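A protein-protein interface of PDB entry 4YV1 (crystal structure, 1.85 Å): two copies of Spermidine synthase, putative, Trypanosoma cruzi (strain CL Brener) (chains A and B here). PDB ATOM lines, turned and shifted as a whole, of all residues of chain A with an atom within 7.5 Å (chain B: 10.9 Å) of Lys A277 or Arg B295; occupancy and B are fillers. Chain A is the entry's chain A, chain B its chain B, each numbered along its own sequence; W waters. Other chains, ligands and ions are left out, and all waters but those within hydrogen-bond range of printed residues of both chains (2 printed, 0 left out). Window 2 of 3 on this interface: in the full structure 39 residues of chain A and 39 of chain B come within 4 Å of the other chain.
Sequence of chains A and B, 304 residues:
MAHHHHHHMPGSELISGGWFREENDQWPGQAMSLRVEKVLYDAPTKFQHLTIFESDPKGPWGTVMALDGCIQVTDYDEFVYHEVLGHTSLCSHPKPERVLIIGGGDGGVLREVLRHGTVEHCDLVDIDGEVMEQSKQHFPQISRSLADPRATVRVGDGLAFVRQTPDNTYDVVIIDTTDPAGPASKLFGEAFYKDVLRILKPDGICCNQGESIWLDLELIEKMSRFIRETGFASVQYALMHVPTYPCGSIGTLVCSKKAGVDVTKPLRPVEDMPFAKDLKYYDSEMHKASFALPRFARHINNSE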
ATOM      1  N   PHE A  79      20.327  13.819  22.431  1.00  0.00           N
ATOM      2  CA  PHE A  79      19.747  14.870  23.296  1.00  0.00           C
ATOM      3  C   PHE A  79      19.064  14.331  24.550  1.00  0.00           C
ATOM      4  O   PHE A  79      18.947  15.051  25.546  1.00  0.00           O
ATOM      5  CB  PHE A  79      18.786  15.786  22.539  1.00  0.00           C
ATOM      6  CG  PHE A  79      17.522  15.073  22.010  1.00  0.00           C
ATOM      7  CD1 PHE A  79      16.353  14.980  22.814  1.00  0.00           C
ATOM      8  CD2 PHE A  79      17.466  14.571  20.697  1.00  0.00           C
ATOM      9  CE1 PHE A  79      15.173  14.330  22.352  1.00  0.00           C
ATOM     10  CE2 PHE A  79      16.282  13.931  20.221  1.00  0.00           C
ATOM     11  CZ  PHE A  79      15.147  13.798  21.041  1.00  0.00           C
ATOM     12  N   GLU A  83      20.426  15.847  27.977  1.00  0.00           N
ATOM     13  CA  GLU A  83      19.536  16.799  28.704  1.00  0.00           C
ATOM     14  C   GLU A  83      19.132  16.242  30.037  1.00  0.00           C
ATOM     15  O   GLU A  83      19.066  16.956  31.013  1.00  0.00           O
ATOM     16  CB  GLU A  83      18.248  17.079  27.943  1.00  0.00           C
ATOM     17  CG  GLU A  83      18.559  17.973  26.711  1.00  0.00           C
ATOM     18  CD  GLU A  83      17.310  18.227  25.878  1.00  0.00           C
ATOM     19  OE1 GLU A  83      16.165  18.026  26.430  1.00  0.00           O
ATOM     20  OE2 GLU A  83      17.477  18.667  24.662  1.00  0.00           O
ATOM     21  N   VAL A 270      13.354  24.644  34.996  1.00  0.00           N
ATOM     22  CA  VAL A 270      13.993  25.073  33.766  1.00  0.00           C
ATOM     23  C   VAL A 270      13.120  26.113  33.013  1.00  0.00           C
ATOM     24  O   VAL A 270      13.656  26.966  32.312  1.00  0.00           O
ATOM     25  CB  VAL A 270      14.416  23.874  32.854  1.00  0.00           C
ATOM     26  CG1 VAL A 270      13.142  23.258  32.214  1.00  0.00           C
ATOM     27  CG2 VAL A 270      15.389  24.332  31.762  1.00  0.00           C
ATOM     28  N   GLU A 271      11.790  26.052  33.165  1.00  0.00           N
ATOM     29  CA  GLU A 271      10.921  27.043  32.499  1.00  0.00           C
ATOM     30  C   GLU A 271      11.253  28.493  32.860  1.00  0.00           C
ATOM     31  O   GLU A 271      10.900  29.416  32.127  1.00  0.00           O
ATOM     32  CB  GLU A 271       9.408  26.769  32.811  1.00  0.00           C
ATOM     33  CG  GLU A 271       8.914  25.450  32.173  1.00  0.00           C
ATOM     34  CD  GLU A 271       9.365  24.202  32.897  1.00  0.00           C
ATOM     35  OE1 GLU A 271       9.802  24.293  34.073  1.00  0.00           O
ATOM     36  OE2 GLU A 271       9.344  23.104  32.285  1.00  0.00           O
ATOM     37  N   MET A 273      14.257  29.703  33.106  1.00  0.00           N
ATOM     38  CA  MET A 273      15.555  30.027  32.525  1.00  0.00           C
ATOM     39  C   MET A 273      15.403  30.304  31.049  1.00  0.00           C
ATOM     40  O   MET A 273      14.458  29.858  30.432  1.00  0.00           O
ATOM     41  CB  MET A 273      16.491  28.848  32.691  1.00  0.00           C
ATOM     42  CG  MET A 273      16.514  28.346  34.120  1.00  0.00           C
ATOM     43  SD  MET A 273      17.589  26.924  34.376  1.00  0.00           S
ATOM     44  CE  MET A 273      17.323  26.649  36.136  1.00  0.00           C
ATOM     45  N   PRO A 274      16.330  31.043  30.446  1.00  0.00           N
ATOM     46  CA  PRO A 274      16.040  31.501  29.102  1.00  0.00           C
ATOM     47  C   PRO A 274      16.216  30.461  27.970  1.00  0.00           C
ATOM     48  O   PRO A 274      15.752  30.698  26.865  1.00  0.00           O
ATOM     49  CB  PRO A 274      17.004  32.697  28.909  1.00  0.00           C
ATOM     50  CG  PRO A 274      18.028  32.562  29.948  1.00  0.00           C
ATOM     51  CD  PRO A 274      17.330  31.892  31.121  1.00  0.00           C
ATOM     52  N   PHE A 275      16.814  29.296  28.258  1.00  0.00           N
ATOM     53  CA  PHE A 275      17.039  28.276  27.223  1.00  0.00           C
ATOM     54  C   PHE A 275      15.994  27.113  27.246  1.00  0.00           C
ATOM     55  O   PHE A 275      16.207  26.104  26.580  1.00  0.00           O
ATOM     56  CB  PHE A 275      18.429  27.686  27.406  1.00  0.00           C
ATOM     57  CG  PHE A 275      18.632  27.023  28.789  1.00  0.00           C
ATOM     58  CD1 PHE A 275      18.300  25.669  29.003  1.00  0.00           C
ATOM     59  CD2 PHE A 275      19.168  27.727  29.840  1.00  0.00           C
ATOM     60  CE1 PHE A 275      18.519  25.071  30.249  1.00  0.00           C
ATOM     61  CE2 PHE A 275      19.375  27.135  31.097  1.00  0.00           C
ATOM     62  CZ  PHE A 275      19.022  25.813  31.307  1.00  0.00           C
ATOM     63  N   ALA A 276      14.952  27.219  28.094  1.00  0.00           N
ATOM     64  CA  ALA A 276      13.942  26.112  28.313  1.00  0.00           C
ATOM     65  C   ALA A 276      13.470  25.596  26.969  1.00  0.00           C
ATOM     66  O   ALA A 276      13.363  24.371  26.739  1.00  0.00           O
ATOM     67  CB  ALA A 276      12.732  26.598  29.140  1.00  0.00           C
ATOM     68  N   LYS A 277      13.147  26.531  26.067  1.00  0.00           N
ATOM     69  CA  LYS A 277      12.600  26.120  24.766  1.00  0.00           C
ATOM     70  C   LYS A 277      13.594  25.597  23.776  1.00  0.00           C
ATOM     71  O   LYS A 277      13.200  25.070  22.752  1.00  0.00           O
ATOM     72  CB  LYS A 277      11.775  27.233  24.143  1.00  0.00           C
ATOM     73  CG  LYS A 277      10.596  27.573  24.993  1.00  0.00           C
ATOM     74  CD  LYS A 277       9.351  27.468  24.145  1.00  0.00           C
ATOM     75  CE  LYS A 277       8.114  27.283  24.985  1.00  0.00           C
ATOM     76  NZ  LYS A 277       7.917  28.480  25.828  1.00  0.00           N
ATOM     77  N   ASP A 278      14.885  25.706  24.043  1.00  0.00           N
ATOM     78  CA  ASP A 278      15.880  25.071  23.172  1.00  0.00           C
ATOM     79  C   ASP A 278      15.972  23.553  23.392  1.00  0.00           C
ATOM     80  O   ASP A 278      16.522  22.819  22.569  1.00  0.00           O
ATOM     81  CB  ASP A 278      17.269  25.639  23.492  1.00  0.00           C
ATOM     82  CG  ASP A 278      17.368  27.101  23.220  1.00  0.00           C
ATOM     83  OD1 ASP A 278      16.516  27.587  22.472  1.00  0.00           O
ATOM     84  OD2 ASP A 278      18.302  27.731  23.759  1.00  0.00           O
ATOM     85  N   LEU A 279      15.439  23.070  24.509  1.00  0.00           N
ATOM     86  CA  LEU A 279      15.555  21.635  24.842  1.00  0.00           C
ATOM     87  C   LEU A 279      14.555  20.799  24.015  1.00  0.00           C
ATOM     88  O   LEU A 279      13.447  21.268  23.690  1.00  0.00           O
ATOM     89  CB  LEU A 279      15.351  21.425  26.361  1.00  0.00           C
ATOM     90  CG  LEU A 279      16.284  22.314  27.237  1.00  0.00           C
ATOM     91  CD1 LEU A 279      16.159  21.922  28.709  1.00  0.00           C
ATOM     92  CD2 LEU A 279      17.739  22.248  26.728  1.00  0.00           C
ATOM     93  N   LYS A 280      14.961  19.589  23.675  1.00  0.00           N
ATOM     94  CA  LYS A 280      14.115  18.706  22.895  1.00  0.00           C
ATOM     95  C   LYS A 280      13.455  17.605  23.693  1.00  0.00           C
ATOM     96  O   LYS A 280      12.542  16.963  23.198  1.00  0.00           O
ATOM     97  CB  LYS A 280      14.970  18.081  21.810  1.00  0.00           C
ATOM     98  CG  LYS A 280      15.465  19.124  20.790  1.00  0.00           C
ATOM     99  CD  LYS A 280      16.636  18.510  19.975  1.00  0.00           C
ATOM    100  CE  LYS A 280      16.786  19.182  18.637  1.00  0.00           C
ATOM    101  NZ  LYS A 280      17.453  20.468  18.971  1.00  0.00           N
ATOM    102  N   TYR A 281      13.919  17.359  24.932  1.00  0.00           N
ATOM    103  CA  TYR A 281      13.312  16.296  25.753  1.00  0.00           C
ATOM    104  C   TYR A 281      12.865  16.873  27.094  1.00  0.00           C
ATOM    105  O   TYR A 281      11.678  16.809  27.414  1.00  0.00           O
ATOM    106  CB  TYR A 281      14.322  15.159  25.957  1.00  0.00           C
ATOM    107  CG  TYR A 281      13.824  13.937  26.744  1.00  0.00           C
ATOM    108  CD1 TYR A 281      13.890  13.893  28.141  1.00  0.00           C
ATOM    109  CD2 TYR A 281      13.252  12.845  26.055  1.00  0.00           C
ATOM    110  CE1 TYR A 281      13.442  12.763  28.850  1.00  0.00           C
ATOM    111  CE2 TYR A 281      12.830  11.688  26.719  1.00  0.00           C
ATOM    112  CZ  TYR A 281      12.911  11.659  28.113  1.00  0.00           C
ATOM    113  OH  TYR A 281      12.502  10.490  28.740  1.00  0.00           O
ATOM    114  N   TYR A 282      13.835  17.378  27.876  1.00  0.00           N
ATOM    115  CA  TYR A 282      13.615  17.732  29.299  1.00  0.00           C
ATOM    116  C   TYR A 282      12.725  18.969  29.519  1.00  0.00           C
ATOM    117  O   TYR A 282      12.826  19.996  28.796  1.00  0.00           O
ATOM    118  CB  TYR A 282      14.984  17.999  29.972  1.00  0.00           C
ATOM    119  CG  TYR A 282      14.896  18.384  31.402  1.00  0.00           C
ATOM    120  CD1 TYR A 282      14.771  19.718  31.759  1.00  0.00           C
ATOM    121  CD2 TYR A 282      14.955  17.391  32.416  1.00  0.00           C
ATOM    122  CE1 TYR A 282      14.724  20.118  33.097  1.00  0.00           C
ATOM    123  CE2 TYR A 282      14.911  17.756  33.749  1.00  0.00           C
ATOM    124  CZ  TYR A 282      14.768  19.106  34.081  1.00  0.00           C
ATOM    125  OH  TYR A 282      14.691  19.527  35.361  1.00  0.00           O
ATOM    126  N   ASP A 283      11.840  18.880  30.488  1.00  0.00           N
ATOM    127  CA  ASP A 283      11.194  20.083  31.065  1.00  0.00           C
ATOM    128  C   ASP A 283      10.768  19.630  32.472  1.00  0.00           C
ATOM    129  O   ASP A 283      11.073  18.478  32.848  1.00  0.00           O
ATOM    130  CB  ASP A 283      10.022  20.648  30.207  1.00  0.00           C
ATOM    131  CG  ASP A 283       8.851  19.652  29.990  1.00  0.00           C
ATOM    132  OD1 ASP A 283       8.693  18.720  30.780  1.00  0.00           O
ATOM    133  OD2 ASP A 283       8.120  19.845  28.973  1.00  0.00           O
ATOM    134  N   SER A 284      10.036  20.476  33.214  1.00  0.00           N
ATOM    135  CA  SER A 284       9.731  20.124  34.606  1.00  0.00           C
ATOM    136  C   SER A 284       8.710  19.018  34.693  1.00  0.00           C
ATOM    137  O   SER A 284       8.754  18.255  35.606  1.00  0.00           O
ATOM    138  CB  SER A 284       9.270  21.338  35.450  1.00  0.00           C
ATOM    139  OG  SER A 284      10.383  22.291  35.565  1.00  0.00           O
ATOM    140  N   MET A 286       8.581  16.452  32.674  1.00  0.00           N
ATOM    141  CA  MET A 286       9.360  15.238  32.392  1.00  0.00           C
ATOM    142  C   MET A 286      10.288  14.904  33.541  1.00  0.00           C
ATOM    143  O   MET A 286      10.571  13.723  33.781  1.00  0.00           O
ATOM    144  CB  MET A 286      10.135  15.366  31.103  1.00  0.00           C
ATOM    145  CG  MET A 286       9.254  15.367  29.794  1.00  0.00           C
ATOM    146  SD  MET A 286       8.499  13.730  29.612  1.00  0.00           S
ATOM    147  CE  MET A 286       9.861  12.687  29.186  1.00  0.00           C
ATOM    148  N   ILE B 213       6.105   7.745  19.418  1.00  0.00           N
ATOM    149  CA  ILE B 213       6.614   9.124  19.248  1.00  0.00           C
ATOM    150  C   ILE B 213       7.942   9.218  18.473  1.00  0.00           C
ATOM    151  O   ILE B 213       8.293  10.307  17.950  1.00  0.00           O
ATOM    152  CB  ILE B 213       6.752   9.863  20.600  1.00  0.00           C
ATOM    153  CG1 ILE B 213       7.885   9.244  21.455  1.00  0.00           C
ATOM    154  CG2 ILE B 213       5.398  10.023  21.269  1.00  0.00           C
ATOM    155  CD1 ILE B 213       8.180  10.066  22.732  1.00  0.00           C
ATOM    156  N   TRP B 214       8.659   8.109  18.331  1.00  0.00           N
ATOM    157  CA  TRP B 214       9.920   8.104  17.612  1.00  0.00           C
ATOM    158  C   TRP B 214       9.669   7.772  16.114  1.00  0.00           C
ATOM    159  O   TRP B 214      10.312   8.325  15.248  1.00  0.00           O
ATOM    160  CB  TRP B 214      10.935   7.089  18.180  1.00  0.00           C
ATOM    161  CG  TRP B 214      11.310   7.420  19.604  1.00  0.00           C
ATOM    162  CD1 TRP B 214      10.821   6.826  20.727  1.00  0.00           C
ATOM    163  CD2 TRP B 214      12.161   8.478  20.023  1.00  0.00           C
ATOM    164  NE1 TRP B 214      11.385   7.417  21.849  1.00  0.00           N
ATOM    165  CE2 TRP B 214      12.216   8.435  21.437  1.00  0.00           C
ATOM    166  CE3 TRP B 214      13.003   9.380  19.333  1.00  0.00           C
ATOM    167  CZ2 TRP B 214      13.031   9.318  22.207  1.00  0.00           C
ATOM    168  CZ3 TRP B 214      13.809  10.309  20.087  1.00  0.00           C
ATOM    169  CH2 TRP B 214      13.813  10.256  21.525  1.00  0.00           C
ATOM    170  N   LEU B 217       5.322   9.925  14.865  1.00  0.00           N
ATOM    171  CA  LEU B 217       4.852  11.123  15.546  1.00  0.00           C
ATOM    172  C   LEU B 217       3.841  11.879  14.655  1.00  0.00           C
ATOM    173  O   LEU B 217       2.859  12.411  15.130  1.00  0.00           O
ATOM    174  CB  LEU B 217       6.027  12.005  15.984  1.00  0.00           C
ATOM    175  CG  LEU B 217       5.619  13.235  16.776  1.00  0.00           C
ATOM    176  CD1 LEU B 217       5.020  12.879  18.159  1.00  0.00           C
ATOM    177  CD2 LEU B 217       6.792  14.207  16.867  1.00  0.00           C
ATOM    178  N   GLU B 221      -0.084  12.873  15.657  1.00  0.00           N
ATOM    179  CA  GLU B 221      -0.660  14.233  15.565  1.00  0.00           C
ATOM    180  C   GLU B 221      -1.967  14.191  14.730  1.00  0.00           C
ATOM    181  O   GLU B 221      -3.000  14.738  15.130  1.00  0.00           O
ATOM    182  CB  GLU B 221       0.340  15.264  14.889  1.00  0.00           C
ATOM    183  CG  GLU B 221       1.760  15.326  15.551  1.00  0.00           C
ATOM    184  CD  GLU B 221       2.940  15.870  14.687  1.00  0.00           C
ATOM    185  OE1 GLU B 221       2.921  15.918  13.407  1.00  0.00           O
ATOM    186  OE2 GLU B 221       3.963  16.245  15.278  1.00  0.00           O
ATOM    187  N   LEU B 239       2.168   7.698  27.142  1.00  0.00           N
ATOM    188  CA  LEU B 239       3.415   7.029  26.753  1.00  0.00           C
ATOM    189  C   LEU B 239       3.778   5.918  27.745  1.00  0.00           C
ATOM    190  O   LEU B 239       3.658   6.083  28.951  1.00  0.00           O
ATOM    191  CB  LEU B 239       4.584   8.089  26.761  1.00  0.00           C
ATOM    192  CG  LEU B 239       5.951   7.724  26.267  1.00  0.00           C
ATOM    193  CD1 LEU B 239       6.043   7.160  24.845  1.00  0.00           C
ATOM    194  CD2 LEU B 239       6.785   9.029  26.354  1.00  0.00           C
ATOM    195  N   PHE B 291       1.390  10.800  30.811  1.00  0.00           N
ATOM    196  CA  PHE B 291       0.917  11.939  29.914  1.00  0.00           C
ATOM    197  C   PHE B 291       1.957  13.054  29.813  1.00  0.00           C
ATOM    198  O   PHE B 291       1.783  13.935  28.981  1.00  0.00           O
ATOM    199  CB  PHE B 291      -0.438  12.501  30.316  1.00  0.00           C
ATOM    200  CG  PHE B 291      -1.542  11.491  30.192  1.00  0.00           C
ATOM    201  CD1 PHE B 291      -2.155  11.272  28.951  1.00  0.00           C
ATOM    202  CD2 PHE B 291      -1.880  10.706  31.284  1.00  0.00           C
ATOM    203  CE1 PHE B 291      -3.169  10.315  28.812  1.00  0.00           C
ATOM    204  CE2 PHE B 291      -2.899   9.743  31.168  1.00  0.00           C
ATOM    205  CZ  PHE B 291      -3.548   9.537  29.932  1.00  0.00           C
ATOM    206  N   ALA B 292       3.076  12.952  30.533  1.00  0.00           N
ATOM    207  CA  ALA B 292       4.203  13.930  30.345  1.00  0.00           C
ATOM    208  C   ALA B 292       5.021  13.429  29.161  1.00  0.00           C
ATOM    209  O   ALA B 292       5.561  12.297  29.186  1.00  0.00           O
ATOM    210  CB  ALA B 292       5.112  14.007  31.592  1.00  0.00           C
ATOM    211  N   LEU B 293       5.085  14.223  28.091  1.00  0.00           N
ATOM    212  CA  LEU B 293       5.831  13.812  26.898  1.00  0.00           C
ATOM    213  C   LEU B 293       7.125  14.641  26.739  1.00  0.00           C
ATOM    214  O   LEU B 293       7.148  15.855  27.101  1.00  0.00           O
ATOM    215  CB  LEU B 293       4.972  14.006  25.626  1.00  0.00           C
ATOM    216  CG  LEU B 293       3.562  13.354  25.654  1.00  0.00           C
ATOM    217  CD1 LEU B 293       2.766  13.603  24.372  1.00  0.00           C
ATOM    218  CD2 LEU B 293       3.610  11.865  26.022  1.00  0.00           C
ATOM    219  N   PRO B 294       8.149  14.026  26.132  1.00  0.00           N
ATOM    220  CA  PRO B 294       9.347  14.754  25.737  1.00  0.00           C
ATOM    221  C   PRO B 294       8.953  15.994  25.022  1.00  0.00           C
ATOM    222  O   PRO B 294       7.912  16.048  24.326  1.00  0.00           O
ATOM    223  CB  PRO B 294      10.068  13.783  24.839  1.00  0.00           C
ATOM    224  CG  PRO B 294       9.597  12.367  25.260  1.00  0.00           C
ATOM    225  CD  PRO B 294       8.174  12.608  25.708  1.00  0.00           C
ATOM    226  N   ARG B 295       9.714  17.058  25.231  1.00  0.00           N
ATOM    227  CA  ARG B 295       9.348  18.332  24.576  1.00  0.00           C
ATOM    228  C   ARG B 295       9.071  18.257  23.083  1.00  0.00           C
ATOM    229  O   ARG B 295       8.104  18.873  22.646  1.00  0.00           O
ATOM    230  CB  ARG B 295      10.454  19.395  24.833  1.00  0.00           C
ATOM    231  CG  ARG B 295      10.254  20.082  26.170  1.00  0.00           C
ATOM    232  CD  ARG B 295      11.000  21.414  26.364  1.00  0.00           C
ATOM    233  NE  ARG B 295      11.026  22.238  25.154  1.00  0.00           N
ATOM    234  CZ  ARG B 295      10.037  23.012  24.764  1.00  0.00           C
ATOM    235  NH1 ARG B 295       8.943  23.097  25.486  1.00  0.00           N
ATOM    236  NH2 ARG B 295      10.136  23.700  23.646  1.00  0.00           N
ATOM    237  N   PHE B 296       9.810  17.447  22.315  1.00  0.00           N
ATOM    238  CA  PHE B 296       9.614  17.432  20.858  1.00  0.00           C
ATOM    239  C   PHE B 296       8.228  16.874  20.517  1.00  0.00           C
ATOM    240  O   PHE B 296       7.682  17.122  19.420  1.00  0.00           O
ATOM    241  CB  PHE B 296      10.719  16.623  20.129  1.00  0.00           C
ATOM    242  CG  PHE B 296      10.636  15.118  20.330  1.00  0.00           C
ATOM    243  CD1 PHE B 296       9.835  14.311  19.501  1.00  0.00           C
ATOM    244  CD2 PHE B 296      11.437  14.499  21.319  1.00  0.00           C
ATOM    245  CE1 PHE B 296       9.784  12.929  19.728  1.00  0.00           C
ATOM    246  CE2 PHE B 296      11.428  13.123  21.534  1.00  0.00           C
ATOM    247  CZ  PHE B 296      10.608  12.341  20.730  1.00  0.00           C
ATOM    248  N   ALA B 297       7.668  16.099  21.449  1.00  0.00           N
ATOM    249  CA  ALA B 297       6.323  15.497  21.218  1.00  0.00           C
ATOM    250  C   ALA B 297       5.198  16.158  22.040  1.00  0.00           C
ATOM    251  O   ALA B 297       4.042  15.766  21.878  1.00  0.00           O
ATOM    252  CB  ALA B 297       6.361  14.007  21.563  1.00  0.00           C
ATOM    253  N   ARG B 298       5.521  17.109  22.914  1.00  0.00           N
ATOM    254  CA  ARG B 298       4.530  17.633  23.895  1.00  0.00           C
ATOM    255  C   ARG B 298       3.276  18.276  23.232  1.00  0.00           C
ATOM    256  O   ARG B 298       2.204  18.315  23.852  1.00  0.00           O
ATOM    257  CB  ARG B 298       5.152  18.665  24.856  1.00  0.00           C
ATOM    258  CG  ARG B 298       5.643  19.933  24.145  1.00  0.00           C
ATOM    259  CD  ARG B 298       5.694  21.252  24.933  1.00  0.00           C
ATOM    260  NE  ARG B 298       6.147  22.501  24.212  1.00  0.00           N
ATOM    261  CZ  ARG B 298       6.079  22.856  22.899  1.00  0.00           C
ATOM    262  NH1 ARG B 298       5.552  22.122  21.922  1.00  0.00           N
ATOM    263  NH2 ARG B 298       6.562  24.047  22.540  1.00  0.00           N
ATOM    264  N   HIS B 299       3.436  18.819  22.020  1.00  0.00           N
ATOM    265  CA  HIS B 299       2.327  19.462  21.291  1.00  0.00           C
ATOM    266  C   HIS B 299       1.168  18.498  21.042  1.00  0.00           C
ATOM    267  O   HIS B 299       0.022  18.962  20.834  1.00  0.00           O
ATOM    268  CB  HIS B 299       2.784  20.094  19.963  1.00  0.00           C
ATOM    269  CG  HIS B 299       3.397  19.126  18.999  1.00  0.00           C
ATOM    270  ND1 HIS B 299       4.689  18.644  19.153  1.00  0.00           N
ATOM    271  CD2 HIS B 299       2.868  18.436  17.963  1.00  0.00           C
ATOM    272  CE1 HIS B 299       4.953  17.774  18.210  1.00  0.00           C
ATOM    273  NE2 HIS B 299       3.874  17.635  17.463  1.00  0.00           N
ATOM    274  N   ILE B 300       1.431  17.172  21.102  1.00  0.00           N
ATOM    275  CA  ILE B 300       0.302  16.193  21.005  1.00  0.00           C
ATOM    276  C   ILE B 300      -0.701  16.499  22.106  1.00  0.00           C
ATOM    277  O   ILE B 300      -1.900  16.358  21.915  1.00  0.00           O
ATOM    278  CB  ILE B 300       0.760  14.704  21.198  1.00  0.00           C
ATOM    279  CG1 ILE B 300       1.835  14.299  20.230  1.00  0.00           C
ATOM    280  CG2 ILE B 300      -0.436  13.776  21.011  1.00  0.00           C
ATOM    281  CD1 ILE B 300       1.517  14.678  18.817  1.00  0.00           C
ATOM    282  N   ASN B 301      -0.196  16.723  23.316  1.00  0.00           N
ATOM    283  CA  ASN B 301      -1.041  16.836  24.501  1.00  0.00           C
ATOM    284  C   ASN B 301      -1.344  18.269  24.959  1.00  0.00           C
ATOM    285  O   ASN B 301      -2.347  18.477  25.671  1.00  0.00           O
ATOM    286  CB  ASN B 301      -0.429  16.077  25.674  1.00  0.00           C
ATOM    287  CG  ASN B 301      -0.636  14.600  25.535  1.00  0.00           C
ATOM    288  OD1 ASN B 301      -1.335  14.187  24.631  1.00  0.00           O
ATOM    289  ND2 ASN B 301      -0.108  13.788  26.493  1.00  0.00           N
ATOM    290  N   ASN B 302      -0.434  19.198  24.601  1.00  0.00           N
ATOM    291  CA  ASN B 302      -0.362  20.619  25.057  1.00  0.00           C
ATOM    292  C   ASN B 302       0.059  21.038  26.500  1.00  0.00           C
ATOM    293  O   ASN B 302       0.075  20.255  27.463  1.00  0.00           O
ATOM    294  CB  ASN B 302      -1.595  21.380  24.595  1.00  0.00           C
ATOM    295  CG  ASN B 302      -1.437  21.892  23.201  1.00  0.00           C
ATOM    296  OD1 ASN B 302      -0.315  21.949  22.676  1.00  0.00           O
ATOM    297  ND2 ASN B 302      -2.545  22.258  22.581  1.00  0.00           N
HETATM  298  O   HOH W   1       6.358  17.868  28.790  1.00  0.00           O
HETATM  299  O   HOH W   2       8.191  22.518  28.082  1.00  0.00           O
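The backbone carbonyl oxygen (O) of Lys A280 sits at hydrogen-bond distance from the backbone NH (N) of Arg B295, 3.5 Å away.
The backbone NH (N) of Phe B296 sits at hydrogen-bond distance from the backbone carbonyl oxygen (O) of Lys A280 (2.9 Å).
O of Tyr A281 lies within hydrogen-bond range of N of Arg B295, 2.9 Å away.
SD of Met A286 lies close to N of Leu B293 (3.8 Å).
NH2 of Arg B295 lies within hydrogen-bond range of O of Lys A277.
The backbone nitrogen of Pro B294 sits close to the side-chain sulfur of Met A286 (3.5 Å).
The backbone carbonyl oxygen (O) of Ala B292 lies close to the side-chain sulfur (SD) of Met A286 (3.3 Å).
The guanidinium group (NE) of Arg B295 sits at hydrogen-bond distance from the backbone carbonyl oxygen (O) of Leu A279 (3.0 Å).
The backbone NH of Tyr A281 is in hydrogen-bond range of the side-chain carboxylate of Glu A83 (2.8 Å).
The backbone NH of Met A286 lies within hydrogen-bond range of the side-chain carboxylate of Asp A283, at 3.0 Å.
A ring nitrogen (ND1) of His B299 lies close to the backbone carbonyl oxygen (O) of Phe B296 (3.4 Å).
N of Tyr A282 is in hydrogen-bond range of OE1 of Glu A83 (2.8 Å).
The side-chain carboxylate (OE2) of Glu A83 sits at hydrogen-bond distance from the backbone NH (N) of Lys A280 (2.9 Å).
Among the printed residues, pairs that only touch across the chains: Tyr A282 with Arg B295, Asp A283 with Arg B295, Tyr A281 with Pro B294, Ala A276 with Arg B295, Phe A79 with Phe B296 and Phe A79 with Trp B214.
Of the printed residues of chain B, Ala A276 touches Arg B295 (3.5 Å).
Of chain B, only Arg B295 comes within 4 Å of Lys A277.
No residue of chain B comes within 4 Å of Asp A278.
Of the printed residues of chain B, Lys A280 touches Arg B295 and Phe B296.
Of the printed residues of chain B, Tyr A282 touches Arg B295.
Printed residues of chain B within 4 Å of Asp A283: Arg B295 (3.5 Å).
Printed residues of chain B within 4 Å of Met A286: Ala B292, Leu B293 and Pro B294.
Of the printed residues of chain A, Trp B214 touches Phe A79 (3.8 Å).
Arg B295 touches seven residues of chain A.
The nearest printed residue of chain A that does not touch Ala B292 is Asp A283 (6.0 Å).
Hydrophobic or aromatic side chains of chain A within 4 Å of the printed part of chain B: Phe A79, Tyr A281 and Met A286.
Of the 17 printed residues of chain B, 6 touch a printed residue of chain A.
Among the printed residues, 14 pairs touch across the chains.
No position is printed for both chains.
Of the 14 pairs that touch across the chains among the printed residues, none has its exchanged pair printed and touching as well.
Water W1 bridges the side-chain carboxylate (OD2) of Asp A283 (2.7 Å) and the backbone carbonyl oxygen (O) of Leu B293 (2.7 Å).
Water W2 bridges the guanidinium group (NH1) of Arg B295 (2.8 Å) and the side-chain carboxylate (OD2) of Asp A283 (2.8 Å).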
